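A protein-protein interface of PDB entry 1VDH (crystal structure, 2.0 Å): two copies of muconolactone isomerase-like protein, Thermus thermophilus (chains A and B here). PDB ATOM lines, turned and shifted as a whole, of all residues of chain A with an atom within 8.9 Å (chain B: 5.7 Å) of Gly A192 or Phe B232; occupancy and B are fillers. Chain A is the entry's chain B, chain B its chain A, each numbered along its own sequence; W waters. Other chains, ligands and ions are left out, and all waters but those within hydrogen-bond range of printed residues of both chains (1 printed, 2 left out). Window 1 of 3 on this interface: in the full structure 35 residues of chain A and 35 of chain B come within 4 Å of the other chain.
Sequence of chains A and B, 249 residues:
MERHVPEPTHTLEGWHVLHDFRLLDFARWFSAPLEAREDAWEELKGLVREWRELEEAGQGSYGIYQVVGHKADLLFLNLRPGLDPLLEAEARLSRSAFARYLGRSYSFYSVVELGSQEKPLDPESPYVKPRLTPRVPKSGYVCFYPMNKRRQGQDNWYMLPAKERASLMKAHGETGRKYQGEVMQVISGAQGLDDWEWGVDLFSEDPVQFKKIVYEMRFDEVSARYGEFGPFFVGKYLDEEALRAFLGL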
ATOM      1  N   SER A 107      -6.167 -22.511 -16.140  1.00  0.00           N
ATOM      2  CA  SER A 107      -7.607 -22.751 -16.122  1.00  0.00           C
ATOM      3  C   SER A 107      -8.348 -21.481 -16.501  1.00  0.00           C
ATOM      4  O   SER A 107      -7.794 -20.376 -16.451  1.00  0.00           O
ATOM      5  CB  SER A 107      -8.067 -23.195 -14.729  1.00  0.00           C
ATOM      6  OG  SER A 107      -8.096 -22.089 -13.834  1.00  0.00           O
ATOM      7  N   PHE A 108      -9.618 -21.636 -16.850  1.00  0.00           N
ATOM      8  CA  PHE A 108     -10.427 -20.487 -17.209  1.00  0.00           C
ATOM      9  C   PHE A 108     -11.892 -20.791 -16.977  1.00  0.00           C
ATOM     10  O   PHE A 108     -12.402 -21.821 -17.422  1.00  0.00           O
ATOM     11  CB  PHE A 108     -10.212 -20.097 -18.675  1.00  0.00           C
ATOM     12  CG  PHE A 108     -10.560 -18.662 -18.979  1.00  0.00           C
ATOM     13  CD1 PHE A 108      -9.743 -17.627 -18.525  1.00  0.00           C
ATOM     14  CD2 PHE A 108     -11.687 -18.345 -19.727  1.00  0.00           C
ATOM     15  CE1 PHE A 108     -10.038 -16.302 -18.815  1.00  0.00           C
ATOM     16  CE2 PHE A 108     -11.997 -17.024 -20.025  1.00  0.00           C
ATOM     17  CZ  PHE A 108     -11.173 -15.997 -19.571  1.00  0.00           C
ATOM     18  N   TYR A 109     -12.545 -19.904 -16.237  1.00  0.00           N
ATOM     19  CA  TYR A 109     -13.971 -20.027 -15.952  1.00  0.00           C
ATOM     20  C   TYR A 109     -14.695 -18.931 -16.721  1.00  0.00           C
ATOM     21  O   TYR A 109     -14.426 -17.743 -16.527  1.00  0.00           O
ATOM     22  CB  TYR A 109     -14.248 -19.874 -14.452  1.00  0.00           C
ATOM     23  CG  TYR A 109     -15.728 -19.772 -14.128  1.00  0.00           C
ATOM     24  CD1 TYR A 109     -16.213 -18.757 -13.304  1.00  0.00           C
ATOM     25  CD2 TYR A 109     -16.648 -20.664 -14.686  1.00  0.00           C
ATOM     26  CE1 TYR A 109     -17.584 -18.629 -13.045  1.00  0.00           C
ATOM     27  CE2 TYR A 109     -18.018 -20.540 -14.436  1.00  0.00           C
ATOM     28  CZ  TYR A 109     -18.477 -19.521 -13.616  1.00  0.00           C
ATOM     29  OH  TYR A 109     -19.830 -19.384 -13.375  1.00  0.00           O
ATOM     30  N   SER A 110     -15.655 -19.329 -17.547  1.00  0.00           N
ATOM     31  CA  SER A 110     -16.406 -18.374 -18.351  1.00  0.00           C
ATOM     32  C   SER A 110     -17.805 -18.889 -18.653  1.00  0.00           C
ATOM     33  O   SER A 110     -18.167 -20.003 -18.270  1.00  0.00           O
ATOM     34  CB  SER A 110     -15.657 -18.097 -19.663  1.00  0.00           C
ATOM     35  OG  SER A 110     -15.469 -19.302 -20.395  1.00  0.00           O
ATOM     36  N   VAL A 111     -18.589 -18.070 -19.349  1.00  0.00           N
ATOM     37  CA  VAL A 111     -19.955 -18.434 -19.697  1.00  0.00           C
ATOM     38  C   VAL A 111     -20.221 -18.077 -21.154  1.00  0.00           C
ATOM     39  O   VAL A 111     -19.947 -16.952 -21.576  1.00  0.00           O
ATOM     40  CB  VAL A 111     -20.983 -17.680 -18.808  1.00  0.00           C
ATOM     41  CG1 VAL A 111     -22.406 -18.084 -19.183  1.00  0.00           C
ATOM     42  CG2 VAL A 111     -20.722 -17.961 -17.321  1.00  0.00           C
ATOM     43  N   ASN A 148      -8.925  -9.501 -23.919  1.00  0.00           N
ATOM     44  CA  ASN A 148      -9.609  -8.323 -23.390  1.00  0.00           C
ATOM     45  C   ASN A 148      -9.781  -7.345 -24.550  1.00  0.00           C
ATOM     46  O   ASN A 148      -9.164  -7.506 -25.605  1.00  0.00           O
ATOM     47  CB  ASN A 148      -8.761  -7.599 -22.342  1.00  0.00           C
ATOM     48  CG  ASN A 148      -8.490  -8.433 -21.116  1.00  0.00           C
ATOM     49  OD1 ASN A 148      -9.346  -9.187 -20.655  1.00  0.00           O
ATOM     50  ND2 ASN A 148      -7.294  -8.277 -20.560  1.00  0.00           N
ATOM     51  N   ARG A 151      -8.322  -0.723 -23.522  1.00  0.00           N
ATOM     52  CA  ARG A 151      -8.779   0.516 -22.897  1.00  0.00           C
ATOM     53  C   ARG A 151      -7.516   1.322 -22.634  1.00  0.00           C
ATOM     54  O   ARG A 151      -7.129   1.527 -21.483  1.00  0.00           O
ATOM     55  CB  ARG A 151      -9.480   0.231 -21.565  1.00  0.00           C
ATOM     56  CG  ARG A 151     -10.850  -0.417 -21.681  1.00  0.00           C
ATOM     57  CD  ARG A 151     -11.453  -0.673 -20.301  1.00  0.00           C
ATOM     58  NE  ARG A 151     -10.580  -1.518 -19.484  1.00  0.00           N
ATOM     59  CZ  ARG A 151      -9.961  -1.116 -18.379  1.00  0.00           C
ATOM     60  NH1 ARG A 151      -9.182  -1.959 -17.717  1.00  0.00           N
ATOM     61  NH2 ARG A 151     -10.131   0.120 -17.922  1.00  0.00           N
ATOM     62  N   GLY A 189     -17.835 -15.277 -22.071  1.00  0.00           N
ATOM     63  CA  GLY A 189     -17.450 -14.093 -21.322  1.00  0.00           C
ATOM     64  C   GLY A 189     -17.018 -14.432 -19.910  1.00  0.00           C
ATOM     65  O   GLY A 189     -17.632 -15.279 -19.263  1.00  0.00           O
ATOM     66  N   ALA A 190     -15.941 -13.803 -19.446  1.00  0.00           N
ATOM     67  CA  ALA A 190     -15.440 -14.039 -18.098  1.00  0.00           C
ATOM     68  C   ALA A 190     -15.347 -12.740 -17.303  1.00  0.00           C
ATOM     69  O   ALA A 190     -14.613 -12.652 -16.310  1.00  0.00           O
ATOM     70  CB  ALA A 190     -14.081 -14.740 -18.146  1.00  0.00           C
ATOM     71  N   GLN A 191     -16.077 -11.724 -17.753  1.00  0.00           N
ATOM     72  CA  GLN A 191     -16.095 -10.432 -17.074  1.00  0.00           C
ATOM     73  C   GLN A 191     -16.602 -10.702 -15.660  1.00  0.00           C
ATOM     74  O   GLN A 191     -17.672 -11.279 -15.482  1.00  0.00           O
ATOM     75  CB  GLN A 191     -17.039  -9.457 -17.785  1.00  0.00           C
ATOM     76  CG  GLN A 191     -16.818  -9.331 -19.298  1.00  0.00           C
ATOM     77  CD  GLN A 191     -17.722 -10.251 -20.111  1.00  0.00           C
ATOM     78  OE1 GLN A 191     -18.098 -11.332 -19.661  1.00  0.00           O
ATOM     79  NE2 GLN A 191     -18.078  -9.816 -21.313  1.00  0.00           N
ATOM     80  N   GLY A 192     -15.795 -10.351 -14.662  1.00  0.00           N
ATOM     81  CA  GLY A 192     -16.182 -10.587 -13.282  1.00  0.00           C
ATOM     82  C   GLY A 192     -16.070 -12.041 -12.843  1.00  0.00           C
ATOM     83  O   GLY A 192     -16.371 -12.360 -11.691  1.00  0.00           O
ATOM     84  N   LEU A 193     -15.605 -12.917 -13.734  1.00  0.00           N
ATOM     85  CA  LEU A 193     -15.488 -14.338 -13.412  1.00  0.00           C
ATOM     86  C   LEU A 193     -14.059 -14.873 -13.448  1.00  0.00           C
ATOM     87  O   LEU A 193     -13.742 -15.844 -12.761  1.00  0.00           O
ATOM     88  CB  LEU A 193     -16.366 -15.169 -14.344  1.00  0.00           C
ATOM     89  CG  LEU A 193     -17.838 -14.753 -14.460  1.00  0.00           C
ATOM     90  CD1 LEU A 193     -18.541 -15.681 -15.448  1.00  0.00           C
ATOM     91  CD2 LEU A 193     -18.515 -14.809 -13.098  1.00  0.00           C
ATOM     92  N   ASP A 194     -13.211 -14.266 -14.271  1.00  0.00           N
ATOM     93  CA  ASP A 194     -11.818 -14.692 -14.362  1.00  0.00           C
ATOM     94  C   ASP A 194     -10.904 -13.521 -14.754  1.00  0.00           C
ATOM     95  O   ASP A 194     -11.366 -12.389 -14.890  1.00  0.00           O
ATOM     96  CB  ASP A 194     -11.669 -15.887 -15.313  1.00  0.00           C
ATOM     97  CG  ASP A 194     -10.639 -16.896 -14.824  1.00  0.00           C
ATOM     98  OD1 ASP A 194     -10.895 -18.113 -14.942  1.00  0.00           O
ATOM     99  OD2 ASP A 194      -9.573 -16.481 -14.316  1.00  0.00           O
ATOM    100  N   ASP A 195      -9.625 -13.810 -14.983  1.00  0.00           N
ATOM    101  CA  ASP A 195      -8.633 -12.778 -15.272  1.00  0.00           C
ATOM    102  C   ASP A 195      -8.716 -12.028 -16.588  1.00  0.00           C
ATOM    103  O   ASP A 195      -8.128 -10.956 -16.724  1.00  0.00           O
ATOM    104  CB  ASP A 195      -7.218 -13.332 -15.068  1.00  0.00           C
ATOM    105  CG  ASP A 195      -6.976 -13.822 -13.647  1.00  0.00           C
ATOM    106  OD1 ASP A 195      -7.915 -13.809 -12.817  1.00  0.00           O
ATOM    107  OD2 ASP A 195      -5.835 -14.239 -13.359  1.00  0.00           O
ATOM    108  N   TRP A 196      -9.448 -12.578 -17.547  1.00  0.00           N
ATOM    109  CA  TRP A 196      -9.609 -11.936 -18.850  1.00  0.00           C
ATOM    110  C   TRP A 196     -11.105 -11.762 -19.107  1.00  0.00           C
ATOM    111  O   TRP A 196     -11.922 -12.496 -18.549  1.00  0.00           O
ATOM    112  CB  TRP A 196      -8.990 -12.801 -19.953  1.00  0.00           C
ATOM    113  CG  TRP A 196      -7.493 -12.988 -19.832  1.00  0.00           C
ATOM    114  CD1 TRP A 196      -6.835 -13.860 -19.009  1.00  0.00           C
ATOM    115  CD2 TRP A 196      -6.480 -12.291 -20.567  1.00  0.00           C
ATOM    116  NE1 TRP A 196      -5.475 -13.749 -19.187  1.00  0.00           N
ATOM    117  CE2 TRP A 196      -5.229 -12.792 -20.138  1.00  0.00           C
ATOM    118  CE3 TRP A 196      -6.507 -11.291 -21.550  1.00  0.00           C
ATOM    119  CZ2 TRP A 196      -4.016 -12.325 -20.655  1.00  0.00           C
ATOM    120  CZ3 TRP A 196      -5.299 -10.825 -22.067  1.00  0.00           C
ATOM    121  CH2 TRP A 196      -4.070 -11.345 -21.617  1.00  0.00           C
ATOM    122  N   GLU A 197     -11.453 -10.827 -19.985  1.00  0.00           N
ATOM    123  CA  GLU A 197     -12.851 -10.542 -20.308  1.00  0.00           C
ATOM    124  C   GLU A 197     -13.567 -11.616 -21.121  1.00  0.00           C
ATOM    125  O   GLU A 197     -14.768 -11.835 -20.947  1.00  0.00           O
ATOM    126  CB  GLU A 197     -12.944  -9.194 -21.009  1.00  0.00           C
ATOM    127  CG  GLU A 197     -12.558  -8.044 -20.103  1.00  0.00           C
ATOM    128  CD  GLU A 197     -12.306  -6.740 -20.839  1.00  0.00           C
ATOM    129  OE1 GLU A 197     -12.100  -5.724 -20.156  1.00  0.00           O
ATOM    130  OE2 GLU A 197     -12.286  -6.722 -22.085  1.00  0.00           O
ATOM    131  N   TRP A 198     -12.842 -12.278 -22.015  1.00  0.00           N
ATOM    132  CA  TRP A 198     -13.435 -13.337 -22.827  1.00  0.00           C
ATOM    133  C   TRP A 198     -12.522 -14.530 -22.966  1.00  0.00           C
ATOM    134  O   TRP A 198     -11.309 -14.435 -22.770  1.00  0.00           O
ATOM    135  CB  TRP A 198     -13.770 -12.850 -24.247  1.00  0.00           C
ATOM    136  CG  TRP A 198     -14.905 -11.873 -24.326  1.00  0.00           C
ATOM    137  CD1 TRP A 198     -16.238 -12.164 -24.394  1.00  0.00           C
ATOM    138  CD2 TRP A 198     -14.803 -10.446 -24.330  1.00  0.00           C
ATOM    139  NE1 TRP A 198     -16.976 -11.004 -24.434  1.00  0.00           N
ATOM    140  CE2 TRP A 198     -16.120  -9.934 -24.396  1.00  0.00           C
ATOM    141  CE3 TRP A 198     -13.728  -9.551 -24.281  1.00  0.00           C
ATOM    142  CZ2 TRP A 198     -16.391  -8.561 -24.412  1.00  0.00           C
ATOM    143  CZ3 TRP A 198     -13.997  -8.182 -24.297  1.00  0.00           C
ATOM    144  CH2 TRP A 198     -15.323  -7.703 -24.361  1.00  0.00           C
ATOM    145  N   LYS B  71      -6.441 -20.957  -9.631  1.00  0.00           N
ATOM    146  CA  LYS B  71      -5.952 -19.859  -8.808  1.00  0.00           C
ATOM    147  C   LYS B  71      -6.076 -20.076  -7.304  1.00  0.00           C
ATOM    148  O   LYS B  71      -5.293 -19.528  -6.537  1.00  0.00           O
ATOM    149  CB  LYS B  71      -6.600 -18.535  -9.226  1.00  0.00           C
ATOM    150  CG  LYS B  71      -6.370 -18.168 -10.698  1.00  0.00           C
ATOM    151  CD  LYS B  71      -6.694 -16.703 -10.970  1.00  0.00           C
ATOM    152  CE  LYS B  71      -8.118 -16.332 -10.571  1.00  0.00           C
ATOM    153  NZ  LYS B  71      -9.152 -16.885 -11.487  1.00  0.00           N
ATOM    154  N   CYS B 143     -17.498 -12.960  -5.391  1.00  0.00           N
ATOM    155  CA  CYS B 143     -16.616 -12.542  -6.471  1.00  0.00           C
ATOM    156  C   CYS B 143     -15.660 -11.544  -5.838  1.00  0.00           C
ATOM    157  O   CYS B 143     -16.099 -10.539  -5.271  1.00  0.00           O
ATOM    158  CB  CYS B 143     -17.375 -11.842  -7.601  1.00  0.00           C
ATOM    159  SG  CYS B 143     -16.284 -10.928  -8.769  1.00  0.00           S
ATOM    160  N   PHE B 144     -14.370 -11.859  -5.861  1.00  0.00           N
ATOM    161  CA  PHE B 144     -13.368 -10.952  -5.315  1.00  0.00           C
ATOM    162  C   PHE B 144     -12.365 -10.548  -6.376  1.00  0.00           C
ATOM    163  O   PHE B 144     -11.883 -11.386  -7.139  1.00  0.00           O
ATOM    164  CB  PHE B 144     -12.580 -11.579  -4.154  1.00  0.00           C
ATOM    165  CG  PHE B 144     -11.348 -10.783  -3.774  1.00  0.00           C
ATOM    166  CD1 PHE B 144     -10.078 -11.194  -4.186  1.00  0.00           C
ATOM    167  CD2 PHE B 144     -11.468  -9.584  -3.081  1.00  0.00           C
ATOM    168  CE1 PHE B 144      -8.953 -10.416  -3.920  1.00  0.00           C
ATOM    169  CE2 PHE B 144     -10.349  -8.795  -2.808  1.00  0.00           C
ATOM    170  CZ  PHE B 144      -9.088  -9.211  -3.231  1.00  0.00           C
ATOM    171  N   TYR B 145     -12.009  -9.270  -6.371  1.00  0.00           N
ATOM    172  CA  TYR B 145     -11.005  -8.749  -7.285  1.00  0.00           C
ATOM    173  C   TYR B 145     -10.442  -7.449  -6.745  1.00  0.00           C
ATOM    174  O   TYR B 145     -11.152  -6.683  -6.088  1.00  0.00           O
ATOM    175  CB  TYR B 145     -11.580  -8.516  -8.688  1.00  0.00           C
ATOM    176  CG  TYR B 145     -12.678  -7.476  -8.769  1.00  0.00           C
ATOM    177  CD1 TYR B 145     -12.390  -6.152  -9.106  1.00  0.00           C
ATOM    178  CD2 TYR B 145     -14.009  -7.826  -8.556  1.00  0.00           C
ATOM    179  CE1 TYR B 145     -13.403  -5.205  -9.233  1.00  0.00           C
ATOM    180  CE2 TYR B 145     -15.027  -6.888  -8.680  1.00  0.00           C
ATOM    181  CZ  TYR B 145     -14.716  -5.582  -9.018  1.00  0.00           C
ATOM    182  OH  TYR B 145     -15.727  -4.660  -9.139  1.00  0.00           O
ATOM    183  N   PRO B 146      -9.124  -7.251  -6.891  1.00  0.00           N
ATOM    184  CA  PRO B 146      -8.483  -6.025  -6.423  1.00  0.00           C
ATOM    185  C   PRO B 146      -8.419  -5.065  -7.617  1.00  0.00           C
ATOM    186  O   PRO B 146      -8.571  -5.489  -8.772  1.00  0.00           O
ATOM    187  CB  PRO B 146      -7.097  -6.515  -6.012  1.00  0.00           C
ATOM    188  CG  PRO B 146      -6.796  -7.538  -7.056  1.00  0.00           C
ATOM    189  CD  PRO B 146      -8.118  -8.287  -7.198  1.00  0.00           C
ATOM    190  N   PHE B 210     -22.549 -11.379 -11.295  1.00  0.00           N
ATOM    191  CA  PHE B 210     -21.214 -10.775 -11.232  1.00  0.00           C
ATOM    192  C   PHE B 210     -20.799 -10.379 -12.651  1.00  0.00           C
ATOM    193  O   PHE B 210     -20.257  -9.292 -12.879  1.00  0.00           O
ATOM    194  CB  PHE B 210     -20.179 -11.776 -10.714  1.00  0.00           C
ATOM    195  CG  PHE B 210     -20.458 -12.306  -9.335  1.00  0.00           C
ATOM    196  CD1 PHE B 210     -20.122 -13.617  -9.013  1.00  0.00           C
ATOM    197  CD2 PHE B 210     -21.009 -11.492  -8.349  1.00  0.00           C
ATOM    198  CE1 PHE B 210     -20.324 -14.116  -7.727  1.00  0.00           C
ATOM    199  CE2 PHE B 210     -21.216 -11.981  -7.057  1.00  0.00           C
ATOM    200  CZ  PHE B 210     -20.873 -13.292  -6.744  1.00  0.00           C
ATOM    201  N   LYS B 211     -21.037 -11.289 -13.595  1.00  0.00           N
ATOM    202  CA  LYS B 211     -20.688 -11.066 -14.998  1.00  0.00           C
ATOM    203  C   LYS B 211     -21.428  -9.872 -15.601  1.00  0.00           C
ATOM    204  O   LYS B 211     -20.827  -9.026 -16.268  1.00  0.00           O
ATOM    205  CB  LYS B 211     -20.975 -12.326 -15.818  1.00  0.00           C
ATOM    206  CG  LYS B 211     -20.587 -12.218 -17.287  1.00  0.00           C
ATOM    207  CD  LYS B 211     -21.016 -13.455 -18.056  1.00  0.00           C
ATOM    208  CE  LYS B 211     -20.625 -13.361 -19.523  1.00  0.00           C
ATOM    209  NZ  LYS B 211     -21.305 -12.234 -20.211  1.00  0.00           N
ATOM    210  N   VAL B 214     -20.210  -6.406 -13.684  1.00  0.00           N
ATOM    211  CA  VAL B 214     -18.831  -6.022 -13.992  1.00  0.00           C
ATOM    212  C   VAL B 214     -18.705  -5.581 -15.453  1.00  0.00           C
ATOM    213  O   VAL B 214     -18.073  -4.568 -15.744  1.00  0.00           O
ATOM    214  CB  VAL B 214     -17.839  -7.161 -13.657  1.00  0.00           C
ATOM    215  CG1 VAL B 214     -16.428  -6.819 -14.150  1.00  0.00           C
ATOM    216  CG2 VAL B 214     -17.815  -7.387 -12.149  1.00  0.00           C
ATOM    217  N   TYR B 215     -19.364  -6.303 -16.358  1.00  0.00           N
ATOM    218  CA  TYR B 215     -19.327  -5.962 -17.781  1.00  0.00           C
ATOM    219  C   TYR B 215     -20.049  -4.637 -18.048  1.00  0.00           C
ATOM    220  O   TYR B 215     -19.508  -3.761 -18.719  1.00  0.00           O
ATOM    221  CB  TYR B 215     -19.946  -7.080 -18.621  1.00  0.00           C
ATOM    222  CG  TYR B 215     -19.739  -6.938 -20.121  1.00  0.00           C
ATOM    223  CD1 TYR B 215     -18.570  -6.369 -20.642  1.00  0.00           C
ATOM    224  CD2 TYR B 215     -20.698  -7.407 -21.017  1.00  0.00           C
ATOM    225  CE1 TYR B 215     -18.362  -6.272 -22.021  1.00  0.00           C
ATOM    226  CE2 TYR B 215     -20.499  -7.318 -22.400  1.00  0.00           C
ATOM    227  CZ  TYR B 215     -19.330  -6.749 -22.892  1.00  0.00           C
ATOM    228  OH  TYR B 215     -19.143  -6.653 -24.255  1.00  0.00           O
ATOM    229  N   ARG B 218     -18.105  -1.557 -16.892  1.00  0.00           N
ATOM    230  CA  ARG B 218     -16.910  -1.211 -17.657  1.00  0.00           C
ATOM    231  C   ARG B 218     -17.198  -0.148 -18.719  1.00  0.00           C
ATOM    232  O   ARG B 218     -16.278   0.506 -19.205  1.00  0.00           O
ATOM    233  CB  ARG B 218     -16.266  -2.461 -18.269  1.00  0.00           C
ATOM    234  CG  ARG B 218     -14.774  -2.283 -18.580  1.00  0.00           C
ATOM    235  CD  ARG B 218     -14.008  -3.585 -18.436  1.00  0.00           C
ATOM    236  NE  ARG B 218     -14.038  -4.075 -17.059  1.00  0.00           N
ATOM    237  CZ  ARG B 218     -13.409  -5.164 -16.629  1.00  0.00           C
ATOM    238  NH1 ARG B 218     -12.676  -5.897 -17.466  1.00  0.00           N
ATOM    239  NH2 ARG B 218     -13.528  -5.533 -15.360  1.00  0.00           N
ATOM    240  N   PHE B 229      -7.834  -3.371 -13.324  1.00  0.00           N
ATOM    241  CA  PHE B 229      -8.260  -4.579 -12.613  1.00  0.00           C
ATOM    242  C   PHE B 229      -7.260  -5.719 -12.461  1.00  0.00           C
ATOM    243  O   PHE B 229      -6.481  -6.001 -13.366  1.00  0.00           O
ATOM    244  CB  PHE B 229      -9.543  -5.112 -13.256  1.00  0.00           C
ATOM    245  CG  PHE B 229     -10.608  -4.064 -13.431  1.00  0.00           C
ATOM    246  CD1 PHE B 229     -11.473  -3.752 -12.389  1.00  0.00           C
ATOM    247  CD2 PHE B 229     -10.714  -3.358 -14.629  1.00  0.00           C
ATOM    248  CE1 PHE B 229     -12.431  -2.746 -12.533  1.00  0.00           C
ATOM    249  CE2 PHE B 229     -11.664  -2.353 -14.785  1.00  0.00           C
ATOM    250  CZ  PHE B 229     -12.525  -2.044 -13.734  1.00  0.00           C
ATOM    251  N   GLY B 230      -7.318  -6.381 -11.304  1.00  0.00           N
ATOM    252  CA  GLY B 230      -6.443  -7.510 -11.028  1.00  0.00           C
ATOM    253  C   GLY B 230      -7.156  -8.832 -11.274  1.00  0.00           C
ATOM    254  O   GLY B 230      -8.115  -8.881 -12.042  1.00  0.00           O
ATOM    255  N   PRO B 231      -6.722  -9.924 -10.629  1.00  0.00           N
ATOM    256  CA  PRO B 231      -7.353 -11.239 -10.809  1.00  0.00           C
ATOM    257  C   PRO B 231      -8.768 -11.311 -10.231  1.00  0.00           C
ATOM    258  O   PRO B 231      -9.093 -10.596  -9.284  1.00  0.00           O
ATOM    259  CB  PRO B 231      -6.398 -12.174 -10.070  1.00  0.00           C
ATOM    260  CG  PRO B 231      -5.861 -11.307  -8.967  1.00  0.00           C
ATOM    261  CD  PRO B 231      -5.594 -10.000  -9.685  1.00  0.00           C
ATOM    262  N   PHE B 232      -9.615 -12.143 -10.836  1.00  0.00           N
ATOM    263  CA  PHE B 232     -10.992 -12.327 -10.373  1.00  0.00           C
ATOM    264  C   PHE B 232     -11.172 -13.750  -9.859  1.00  0.00           C
ATOM    265  O   PHE B 232     -10.836 -14.717 -10.552  1.00  0.00           O
ATOM    266  CB  PHE B 232     -12.003 -12.059 -11.501  1.00  0.00           C
ATOM    267  CG  PHE B 232     -12.190 -10.601 -11.825  1.00  0.00           C
ATOM    268  CD1 PHE B 232     -11.210  -9.891 -12.509  1.00  0.00           C
ATOM    269  CD2 PHE B 232     -13.349  -9.936 -11.438  1.00  0.00           C
ATOM    270  CE1 PHE B 232     -11.383  -8.533 -12.802  1.00  0.00           C
ATOM    271  CE2 PHE B 232     -13.532  -8.582 -11.725  1.00  0.00           C
ATOM    272  CZ  PHE B 232     -12.549  -7.880 -12.406  1.00  0.00           C
ATOM    273  N   PHE B 233     -11.679 -13.868  -8.635  1.00  0.00           N
ATOM    274  CA  PHE B 233     -11.911 -15.168  -8.004  1.00  0.00           C
ATOM    275  C   PHE B 233     -13.396 -15.348  -7.736  1.00  0.00           C
ATOM    276  O   PHE B 233     -14.046 -14.448  -7.205  1.00  0.00           O
ATOM    277  CB  PHE B 233     -11.199 -15.259  -6.649  1.00  0.00           C
ATOM    278  CG  PHE B 233      -9.702 -15.192  -6.729  1.00  0.00           C
ATOM    279  CD1 PHE B 233      -8.939 -16.347  -6.641  1.00  0.00           C
ATOM    280  CD2 PHE B 233      -9.052 -13.966  -6.839  1.00  0.00           C
ATOM    281  CE1 PHE B 233      -7.547 -16.285  -6.656  1.00  0.00           C
ATOM    282  CE2 PHE B 233      -7.669 -13.895  -6.854  1.00  0.00           C
ATOM    283  CZ  PHE B 233      -6.912 -15.057  -6.762  1.00  0.00           C
ATOM    284  N   VAL B 234     -13.933 -16.504  -8.100  1.00  0.00           N
ATOM    285  CA  VAL B 234     -15.342 -16.778  -7.843  1.00  0.00           C
ATOM    286  C   VAL B 234     -15.436 -18.007  -6.952  1.00  0.00           C
ATOM    287  O   VAL B 234     -14.808 -19.030  -7.222  1.00  0.00           O
ATOM    288  CB  VAL B 234     -16.153 -17.011  -9.134  1.00  0.00           C
ATOM    289  CG1 VAL B 234     -17.619 -17.279  -8.782  1.00  0.00           C
ATOM    290  CG2 VAL B 234     -16.069 -15.790 -10.042  1.00  0.00           C
HETATM  291  O   HOH W   1      -7.187  -3.532 -16.145  1.00  0.00           O
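Of the 16 printed residues of chain B, 11 touch a printed residue of chain A.
Hydrophobic or aromatic side chains of chain B within 4 Å of the printed part of chain A: Phe B210, Val B214, Tyr B215, Phe B229, Pro B231, Phe B232 and Val B234.
Printed residues of chain A that touch a printed residue of chain B: Arg A151, Gly A189, Gln A191, Gly A192, Leu A193, Asp A194, Asp A195, Glu A197 and Trp A198.
Among the printed residues, Asp or Glu carboxylates within 4 Å of a Lys or Arg side-chain nitrogen of the other chain: Asp A194 with Lys B71 (2.9 Å), Asp A195 with Lys B71 (3.6 Å) and Glu A197 with Arg B218 (2.8 Å).
Water W1 bridges the backbone NH of Phe B229 (2.9 Å) and the guanidinium group of Arg A151 (3.0 Å).
No position is printed for both chains.
Of chain B, only Cys B143 (3.3 Å), Phe B210 (3.97 Å), Val B214 (3.6 Å), Phe B232 (3.4 Å) and Val B234 (3.8 Å) come within 4 Å of Gly A192.
Of chain A, only Gly A192 (3.4 Å), Leu A193 (3.8 Å), Asp A194 (3.5 Å) and Asp A195 (3.1 Å) come within 4 Å of Phe B232.
Pro B231 touches just one residue of chain A: Asp A195.
Of the printed residues of chain A, Tyr B215 touches Gln A191 and Trp A198.
Printed residues of chain B within 4 Å of Glu A197: Arg B218 (2.8 Å).
Val A111 touches none of the printed residues of chain B.
The nearest residue of chain B that does not touch Gly A192 is Lys B211 (4.8 Å).
The nearest printed residue of chain A that does not touch Lys B71 is Ser A107 (4.7 Å).
OD2 of Asp A194 lies within salt-bridge range of NZ of Lys B71 (2.9 Å).
The side-chain carboxylate (OD1) of Asp A195 lies within salt-bridge range of the side-chain amino group (NZ) of Lys B71 (3.6 Å).
The side-chain sulfur (SG) of Cys B143 sits at hydrogen-bond distance from the backbone carbonyl oxygen (O) of Gly A192 (3.3 Å).
The side-chain amino group (NZ) of Lys B211 sits close to the side-chain amide oxygen (OE1) of Gln A191, at 3.4 Å.
NH1 of Arg B218 is in salt-bridge range of OE1 of Glu A197, 2.8 Å away.
OD1 of Asp A195 is in hydrogen-bond range of N of Phe B232, at 3.1 Å.
NZ of Lys B71 sits at hydrogen-bond distance from O of Phe B232 (2.9 Å).
The side-chain carboxylate of Asp A194 is in hydrogen-bond range of the backbone NH of Tyr A109, at 2.8 Å.
N of Gly A189 is in hydrogen-bond range of O of Val A111, 2.7 Å away.
The side-chain amide oxygen of Asn A148 is in hydrogen-bond range of the backbone NH of Glu A197.
The backbone NH (N) of Ala A190 is in hydrogen-bond range of the backbone carbonyl oxygen (O) of Glu A197, at 2.7 Å.
The backbone carbonyl oxygen (O) of Glu A197 sits at hydrogen-bond distance from the backbone NH (N) of Gln A191.
CD2 of Phe B229 touches NH1 of Arg A151, 3.7 Å away.
Lys B211 touches Gly A189.
Tyr B215 touches Gln A191.
Phe B210 touches Gly A192 (CB to O, 3.97 Å).
Gly A192 touches Val B214.
Phe B232 touches Gly A192.
O of Leu A193 touches O of Phe B232 (3.8 Å).
O of Asp A194 touches CD1 of Phe B232, 3.5 Å away.
CA of Pro B231 touches OD1 of Asp A195, 3.3 Å away.
Tyr B215 touches Trp A198 (OH to CZ2, 3.4 Å).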
